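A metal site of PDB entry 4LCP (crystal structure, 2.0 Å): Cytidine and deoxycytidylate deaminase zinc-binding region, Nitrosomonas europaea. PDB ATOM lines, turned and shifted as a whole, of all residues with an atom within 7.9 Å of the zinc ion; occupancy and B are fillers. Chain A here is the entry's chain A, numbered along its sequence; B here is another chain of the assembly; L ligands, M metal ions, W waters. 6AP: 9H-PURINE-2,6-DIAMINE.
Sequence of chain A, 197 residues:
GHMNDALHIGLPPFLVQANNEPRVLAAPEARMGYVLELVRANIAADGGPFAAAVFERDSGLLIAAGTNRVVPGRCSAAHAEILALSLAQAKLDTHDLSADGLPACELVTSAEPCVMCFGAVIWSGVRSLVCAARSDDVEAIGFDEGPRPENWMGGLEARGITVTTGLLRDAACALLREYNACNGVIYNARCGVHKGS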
ATOM      1  N   PHE A  50      25.276   1.516 -26.735  1.00  0.00           N
ATOM      2  CA  PHE A  50      24.325   2.381 -27.450  1.00  0.00           C
ATOM      3  C   PHE A  50      24.780   3.803 -27.296  1.00  0.00           C
ATOM      4  O   PHE A  50      25.276   4.197 -26.214  1.00  0.00           O
ATOM      5  CB  PHE A  50      22.898   2.243 -26.848  1.00  0.00           C
ATOM      6  CG  PHE A  50      22.340   0.890 -26.983  1.00  0.00           C
ATOM      7  CD1 PHE A  50      21.887   0.448 -28.242  1.00  0.00           C
ATOM      8  CD2 PHE A  50      22.267   0.035 -25.885  1.00  0.00           C
ATOM      9  CE1 PHE A  50      21.347  -0.860 -28.363  1.00  0.00           C
ATOM     10  CE2 PHE A  50      21.724  -1.243 -26.027  1.00  0.00           C
ATOM     11  CZ  PHE A  50      21.317  -1.695 -27.254  1.00  0.00           C
ATOM     12  N   ASN A  68      24.258   5.336 -23.466  1.00  0.00           N
ATOM     13  CA  ASN A  68      23.437   4.694 -22.447  1.00  0.00           C
ATOM     14  C   ASN A  68      24.150   4.709 -21.067  1.00  0.00           C
ATOM     15  O   ASN A  68      25.259   4.163 -20.926  1.00  0.00           O
ATOM     16  CB  ASN A  68      22.991   3.374 -22.954  1.00  0.00           C
ATOM     17  CG  ASN A  68      22.367   2.246 -22.151  1.00  0.00           C
ATOM     18  OD1 ASN A  68      22.667   2.042 -20.988  1.00  0.00           O
ATOM     19  ND2 ASN A  68      21.501   1.484 -22.784  1.00  0.00           N
ATOM     20  N   VAL A  70      22.335   3.921 -18.188  1.00  0.00           N
ATOM     21  CA  VAL A  70      21.316   3.273 -17.314  1.00  0.00           C
ATOM     22  C   VAL A  70      21.950   2.757 -15.998  1.00  0.00           C
ATOM     23  O   VAL A  70      21.543   3.198 -14.894  1.00  0.00           O
ATOM     24  CB  VAL A  70      20.578   2.173 -18.110  1.00  0.00           C
ATOM     25  CG1 VAL A  70      19.683   1.264 -17.242  1.00  0.00           C
ATOM     26  CG2 VAL A  70      19.798   2.839 -19.215  1.00  0.00           C
ATOM     27  N   SER A  76      16.816   4.274 -15.387  1.00  0.00           N
ATOM     28  CA  SER A  76      16.392   3.478 -16.498  1.00  0.00           C
ATOM     29  C   SER A  76      15.990   4.366 -17.706  1.00  0.00           C
ATOM     30  O   SER A  76      15.960   3.895 -18.836  1.00  0.00           O
ATOM     31  CB  SER A  76      15.265   2.503 -16.079  1.00  0.00           C
ATOM     32  OG  SER A  76      14.150   3.292 -15.659  1.00  0.00           O
ATOM     33  N   ALA A  77      15.691   5.650 -17.461  1.00  0.00           N
ATOM     34  CA  ALA A  77      15.426   6.555 -18.573  1.00  0.00           C
ATOM     35  C   ALA A  77      16.662   6.991 -19.326  1.00  0.00           C
ATOM     36  O   ALA A  77      16.523   7.612 -20.343  1.00  0.00           O
ATOM     37  CB  ALA A  77      14.670   7.806 -18.105  1.00  0.00           C
ATOM     38  N   ALA A  78      17.850   6.617 -18.872  1.00  0.00           N
ATOM     39  CA  ALA A  78      19.092   7.211 -19.431  1.00  0.00           C
ATOM     40  C   ALA A  78      19.606   6.467 -20.693  1.00  0.00           C
ATOM     41  O   ALA A  78      20.762   6.031 -20.758  1.00  0.00           O
ATOM     42  CB  ALA A  78      20.178   7.234 -18.368  1.00  0.00           C
ATOM     43  N   HIS A  79      18.719   6.268 -21.645  1.00  0.00           N
ATOM     44  CA  HIS A  79      19.099   5.705 -22.938  1.00  0.00           C
ATOM     45  C   HIS A  79      19.863   6.742 -23.702  1.00  0.00           C
ATOM     46  O   HIS A  79      19.762   7.912 -23.414  1.00  0.00           O
ATOM     47  CB  HIS A  79      17.886   5.287 -23.724  1.00  0.00           C
ATOM     48  CG  HIS A  79      17.251   4.035 -23.209  1.00  0.00           C
ATOM     49  ND1 HIS A  79      16.405   3.286 -23.960  1.00  0.00           N
ATOM     50  CD2 HIS A  79      17.350   3.389 -21.956  1.00  0.00           C
ATOM     51  CE1 HIS A  79      15.989   2.214 -23.230  1.00  0.00           C
ATOM     52  NE2 HIS A  79      16.596   2.268 -22.023  1.00  0.00           N
ATOM     53  N   ALA A  80      20.675   6.327 -24.663  1.00  0.00           N
ATOM     54  CA  ALA A  80      21.546   7.242 -25.427  1.00  0.00           C
ATOM     55  C   ALA A  80      20.720   8.382 -26.064  1.00  0.00           C
ATOM     56  O   ALA A  80      21.153   9.564 -26.115  1.00  0.00           O
ATOM     57  CB  ALA A  80      22.204   6.455 -26.550  1.00  0.00           C
ATOM     58  N   GLU A  81      19.565   8.008 -26.595  1.00  0.00           N
ATOM     59  CA  GLU A  81      18.677   8.956 -27.326  1.00  0.00           C
ATOM     60  C   GLU A  81      18.168  10.072 -26.400  1.00  0.00           C
ATOM     61  O   GLU A  81      18.103  11.254 -26.793  1.00  0.00           O
ATOM     62  CB  GLU A  81      17.466   8.199 -27.905  1.00  0.00           C
ATOM     63  CG  GLU A  81      17.828   7.126 -28.905  1.00  0.00           C
ATOM     64  CD  GLU A  81      17.906   5.767 -28.260  1.00  0.00           C
ATOM     65  OE1 GLU A  81      18.657   5.601 -27.263  1.00  0.00           O
ATOM     66  OE2 GLU A  81      17.237   4.835 -28.803  1.00  0.00           O
ATOM     67  N   ILE A  82      17.758   9.703 -25.196  1.00  0.00           N
ATOM     68  CA  ILE A  82      17.219  10.644 -24.194  1.00  0.00           C
ATOM     69  C   ILE A  82      18.353  11.597 -23.771  1.00  0.00           C
ATOM     70  O   ILE A  82      18.144  12.803 -23.694  1.00  0.00           O
ATOM     71  CB  ILE A  82      16.762   9.938 -22.880  1.00  0.00           C
ATOM     72  CG1 ILE A  82      15.633   8.921 -23.176  1.00  0.00           C
ATOM     73  CG2 ILE A  82      16.239  10.980 -21.897  1.00  0.00           C
ATOM     74  CD1 ILE A  82      14.517   9.448 -24.069  1.00  0.00           C
ATOM     75  N   THR A 109      21.705   7.526 -34.368  1.00  0.00           N
ATOM     76  CA  THR A 109      21.632   6.640 -33.236  1.00  0.00           C
ATOM     77  C   THR A 109      22.154   5.259 -33.656  1.00  0.00           C
ATOM     78  O   THR A 109      21.940   4.759 -34.800  1.00  0.00           O
ATOM     79  CB  THR A 109      20.190   6.620 -32.701  1.00  0.00           C
ATOM     80  OG1 THR A 109      20.107   5.768 -31.532  1.00  0.00           O
ATOM     81  CG2 THR A 109      19.259   5.996 -33.818  1.00  0.00           C
ATOM     82  N   ALA A 111      21.409   2.424 -32.990  1.00  0.00           N
ATOM     83  CA  ALA A 111      20.349   1.367 -33.055  1.00  0.00           C
ATOM     84  C   ALA A 111      18.913   1.975 -33.134  1.00  0.00           C
ATOM     85  O   ALA A 111      18.645   3.035 -32.572  1.00  0.00           O
ATOM     86  CB  ALA A 111      20.450   0.439 -31.815  1.00  0.00           C
ATOM     87  N   GLU A 112      17.966   1.243 -33.732  1.00  0.00           N
ATOM     88  CA  GLU A 112      16.550   1.649 -33.741  1.00  0.00           C
ATOM     89  C   GLU A 112      16.001   1.873 -32.322  1.00  0.00           C
ATOM     90  O   GLU A 112      16.365   1.138 -31.401  1.00  0.00           O
ATOM     91  CB  GLU A 112      15.717   0.610 -34.503  1.00  0.00           C
ATOM     92  CG  GLU A 112      16.111   0.676 -36.023  1.00  0.00           C
ATOM     93  CD  GLU A 112      15.325  -0.326 -36.866  1.00  0.00           C
ATOM     94  OE1 GLU A 112      14.574  -1.154 -36.236  1.00  0.00           O
ATOM     95  OE2 GLU A 112      15.496  -0.325 -38.120  1.00  0.00           O
ATOM     96  N   PRO A 113      15.201   2.948 -32.138  1.00  0.00           N
ATOM     97  CA  PRO A 113      14.833   3.360 -30.832  1.00  0.00           C
ATOM     98  C   PRO A 113      13.854   2.385 -30.155  1.00  0.00           C
ATOM     99  O   PRO A 113      13.029   1.715 -30.837  1.00  0.00           O
ATOM    100  CB  PRO A 113      14.257   4.785 -31.052  1.00  0.00           C
ATOM    101  CG  PRO A 113      13.596   4.674 -32.398  1.00  0.00           C
ATOM    102  CD  PRO A 113      14.678   3.869 -33.161  1.00  0.00           C
ATOM    103  N   CYS A 114      13.933   2.266 -28.824  1.00  0.00           N
ATOM    104  CA  CYS A 114      12.935   1.454 -28.074  1.00  0.00           C
ATOM    105  C   CYS A 114      11.631   2.279 -28.035  1.00  0.00           C
ATOM    106  O   CYS A 114      11.638   3.472 -28.462  1.00  0.00           O
ATOM    107  CB  CYS A 114      13.486   1.156 -26.659  1.00  0.00           C
ATOM    108  SG  CYS A 114      13.359   2.633 -25.548  1.00  0.00           S
ATOM    109  N   VAL A 115      10.531   1.740 -27.462  1.00  0.00           N
ATOM    110  CA  VAL A 115       9.280   2.542 -27.464  1.00  0.00           C
ATOM    111  C   VAL A 115       9.404   3.881 -26.692  1.00  0.00           C
ATOM    112  O   VAL A 115       8.796   4.874 -27.126  1.00  0.00           O
ATOM    113  CB  VAL A 115       8.066   1.733 -26.972  1.00  0.00           C
ATOM    114  CG1 VAL A 115       8.322   1.221 -25.558  1.00  0.00           C
ATOM    115  CG2 VAL A 115       6.776   2.554 -27.068  1.00  0.00           C
ATOM    116  N   MET A 116      10.138   3.925 -25.575  1.00  0.00           N
ATOM    117  CA  MET A 116      10.302   5.173 -24.823  1.00  0.00           C
ATOM    118  C   MET A 116      11.010   6.242 -25.692  1.00  0.00           C
ATOM    119  O   MET A 116      10.558   7.396 -25.810  1.00  0.00           O
ATOM    120  CB  MET A 116      11.132   4.903 -23.547  1.00  0.00           C
ATOM    121  CG  MET A 116      11.573   6.146 -22.763  1.00  0.00           C
ATOM    122  SD  MET A 116      12.605   5.721 -21.316  1.00  0.00           S
ATOM    123  CE  MET A 116      14.145   5.237 -22.149  1.00  0.00           C
ATOM    124  N   CYS A 117      12.126   5.820 -26.295  1.00  0.00           N
ATOM    125  CA  CYS A 117      12.944   6.678 -27.147  1.00  0.00           C
ATOM    126  C   CYS A 117      12.211   7.135 -28.402  1.00  0.00           C
ATOM    127  O   CYS A 117      12.366   8.271 -28.866  1.00  0.00           O
ATOM    128  CB  CYS A 117      14.318   6.042 -27.389  1.00  0.00           C
ATOM    129  SG  CYS A 117      15.324   6.029 -25.859  1.00  0.00           S
ATOM    130  N   PHE A 118      11.377   6.239 -28.936  1.00  0.00           N
ATOM    131  CA  PHE A 118      10.505   6.557 -30.036  1.00  0.00           C
ATOM    132  C   PHE A 118       9.613   7.766 -29.718  1.00  0.00           C
ATOM    133  O   PHE A 118       9.502   8.693 -30.525  1.00  0.00           O
ATOM    134  CB  PHE A 118       9.640   5.309 -30.312  1.00  0.00           C
ATOM    135  CG  PHE A 118       8.452   5.534 -31.199  1.00  0.00           C
ATOM    136  CD1 PHE A 118       8.592   5.708 -32.571  1.00  0.00           C
ATOM    137  CD2 PHE A 118       7.197   5.462 -30.670  1.00  0.00           C
ATOM    138  CE1 PHE A 118       7.456   5.883 -33.363  1.00  0.00           C
ATOM    139  CE2 PHE A 118       6.088   5.611 -31.465  1.00  0.00           C
ATOM    140  CZ  PHE A 118       6.197   5.822 -32.812  1.00  0.00           C
ATOM    141  N   ALA A 120      10.235   9.882 -27.269  1.00  0.00           N
ATOM    142  CA  ALA A 120      11.146  11.055 -27.046  1.00  0.00           C
ATOM    143  C   ALA A 120      11.527  11.767 -28.341  1.00  0.00           C
ATOM    144  O   ALA A 120      11.639  13.026 -28.413  1.00  0.00           O
ATOM    145  CB  ALA A 120      12.428  10.641 -26.262  1.00  0.00           C
ATOM    146  N   ASP A 144      15.561  -5.363 -25.293  1.00  0.00           N
ATOM    147  CA  ASP A 144      14.137  -5.464 -25.631  1.00  0.00           C
ATOM    148  C   ASP A 144      13.752  -4.096 -26.176  1.00  0.00           C
ATOM    149  O   ASP A 144      14.048  -3.076 -25.557  1.00  0.00           O
ATOM    150  CB  ASP A 144      13.376  -5.749 -24.339  1.00  0.00           C
ATOM    151  CG  ASP A 144      11.888  -5.892 -24.514  1.00  0.00           C
ATOM    152  OD1 ASP A 144      11.265  -5.756 -25.622  1.00  0.00           O
ATOM    153  OD2 ASP A 144      11.311  -6.159 -23.441  1.00  0.00           O
ATOM    154  N   GLU A 145      13.148  -4.066 -27.339  1.00  0.00           N
ATOM    155  CA  GLU A 145      12.713  -2.788 -27.880  1.00  0.00           C
ATOM    156  C   GLU A 145      11.389  -2.335 -27.234  1.00  0.00           C
ATOM    157  O   GLU A 145      11.040  -1.148 -27.290  1.00  0.00           O
ATOM    158  CB  GLU A 145      12.637  -2.867 -29.406  1.00  0.00           C
ATOM    159  CG  GLU A 145      14.074  -3.032 -29.999  1.00  0.00           C
ATOM    160  CD  GLU A 145      14.835  -1.686 -30.131  1.00  0.00           C
ATOM    161  OE1 GLU A 145      14.887  -0.907 -29.127  1.00  0.00           O
ATOM    162  OE2 GLU A 145      15.377  -1.366 -31.244  1.00  0.00           O
ATOM    163  N   TRP B 123      10.403   0.153 -18.362  1.00  0.00           N
ATOM    164  CA  TRP B 123      11.828  -0.173 -18.076  1.00  0.00           C
ATOM    165  C   TRP B 123      12.060   0.084 -16.655  1.00  0.00           C
ATOM    166  O   TRP B 123      13.073  -0.314 -16.154  1.00  0.00           O
ATOM    167  CB  TRP B 123      12.834   0.698 -18.900  1.00  0.00           C
ATOM    168  CG  TRP B 123      12.613   0.627 -20.392  1.00  0.00           C
ATOM    169  CD1 TRP B 123      12.607   1.683 -21.326  1.00  0.00           C
ATOM    170  CD2 TRP B 123      12.301  -0.566 -21.158  1.00  0.00           C
ATOM    171  NE1 TRP B 123      12.331   1.210 -22.598  1.00  0.00           N
ATOM    172  CE2 TRP B 123      12.117  -0.136 -22.555  1.00  0.00           C
ATOM    173  CE3 TRP B 123      12.133  -1.918 -20.815  1.00  0.00           C
ATOM    174  CZ2 TRP B 123      11.798  -1.049 -23.571  1.00  0.00           C
ATOM    175  CZ3 TRP B 123      11.856  -2.825 -21.814  1.00  0.00           C
ATOM    176  CH2 TRP B 123      11.666  -2.409 -23.176  1.00  0.00           C
HETATM  177  N9  6AP L   1      19.282   1.145 -24.209  1.00  0.00           N
HETATM  178  C8  6AP L   1      18.911   0.375 -23.179  1.00  0.00           C
HETATM  179  N7  6AP L   1      18.010  -0.547 -23.562  1.00  0.00           N
HETATM  180  C5  6AP L   1      17.846  -0.333 -24.934  1.00  0.00           C
HETATM  181  C4  6AP L   1      18.644   0.715 -25.334  1.00  0.00           C
HETATM  182  N3  6AP L   1      18.657   1.106 -26.646  1.00  0.00           N
HETATM  183  C2  6AP L   1      17.923   0.507 -27.593  1.00  0.00           C
HETATM  184  N2  6AP L   1      18.029   0.987 -28.973  1.00  0.00           N
HETATM  185  N1  6AP L   1      17.122  -0.511 -27.214  1.00  0.00           N
HETATM  186  C6  6AP L   1      17.062  -0.942 -25.922  1.00  0.00           C
HETATM  187  N6  6AP L   1      16.250  -2.000 -25.432  1.00  0.00           N
HETATM  188 ZN    ZN M   1      15.339   3.749 -25.608  1.00  0.00          ZN
HETATM  189  O   HOH W   1      16.322   3.024 -27.396  1.00  0.00           O
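Water W1 lies within hydrogen-bond range of OE2 of Glu 81 (2.5 Å), N of Cys 114 (2.9 Å) and N2 of the ligand (3.1 Å).
The indole nitrogen of Trp 123 of chain B lies close to the side-chain sulfur of Cys 114 (3.4 Å). The backbone NH of Cys 114 lies close to the side-chain carboxylate of Glu 145 (3.3 Å). The side-chain sulfur (SG) of Cys 114 sits close to the backbone NH (N) of Met 116 (3.5 Å). SG of Cys 117 sits close to OE1 of Glu 81 (3.6 Å).
O of Asp 144 sits at hydrogen-bond distance from N6 of the ligand (2.5 Å). The backbone carbonyl oxygen of Glu 112 lies within hydrogen-bond range of a nitrogen (N2) of the ligand (2.9 Å). N9 of the ligand sits close to ND2 of Asn 68.
A ring nitrogen (ND1) of His 79 binds the zinc ion (2.0 Å). Water W1 binds the zinc ion, 2.2 Å away. The side-chain sulfur (SG) of Cys 114 is bound to the zinc ion. The side-chain sulfur (SG) of Cys 117 binds the zinc ion (2.3 Å). The zinc ion has four donor atoms within binding distance.
OE2 of Glu 81 touches the zinc ion (3.9 Å). Met 116 touches the zinc ion (CE to ZN, 3.95 Å). Five residues have an atom within 4 Å of the zinc ion: His 79, Glu 81, Cys 114, Met 116 and Cys 117. The nearest printed residue that does not touch the zinc ion is Trp 123 of chain B (5.0 Å).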
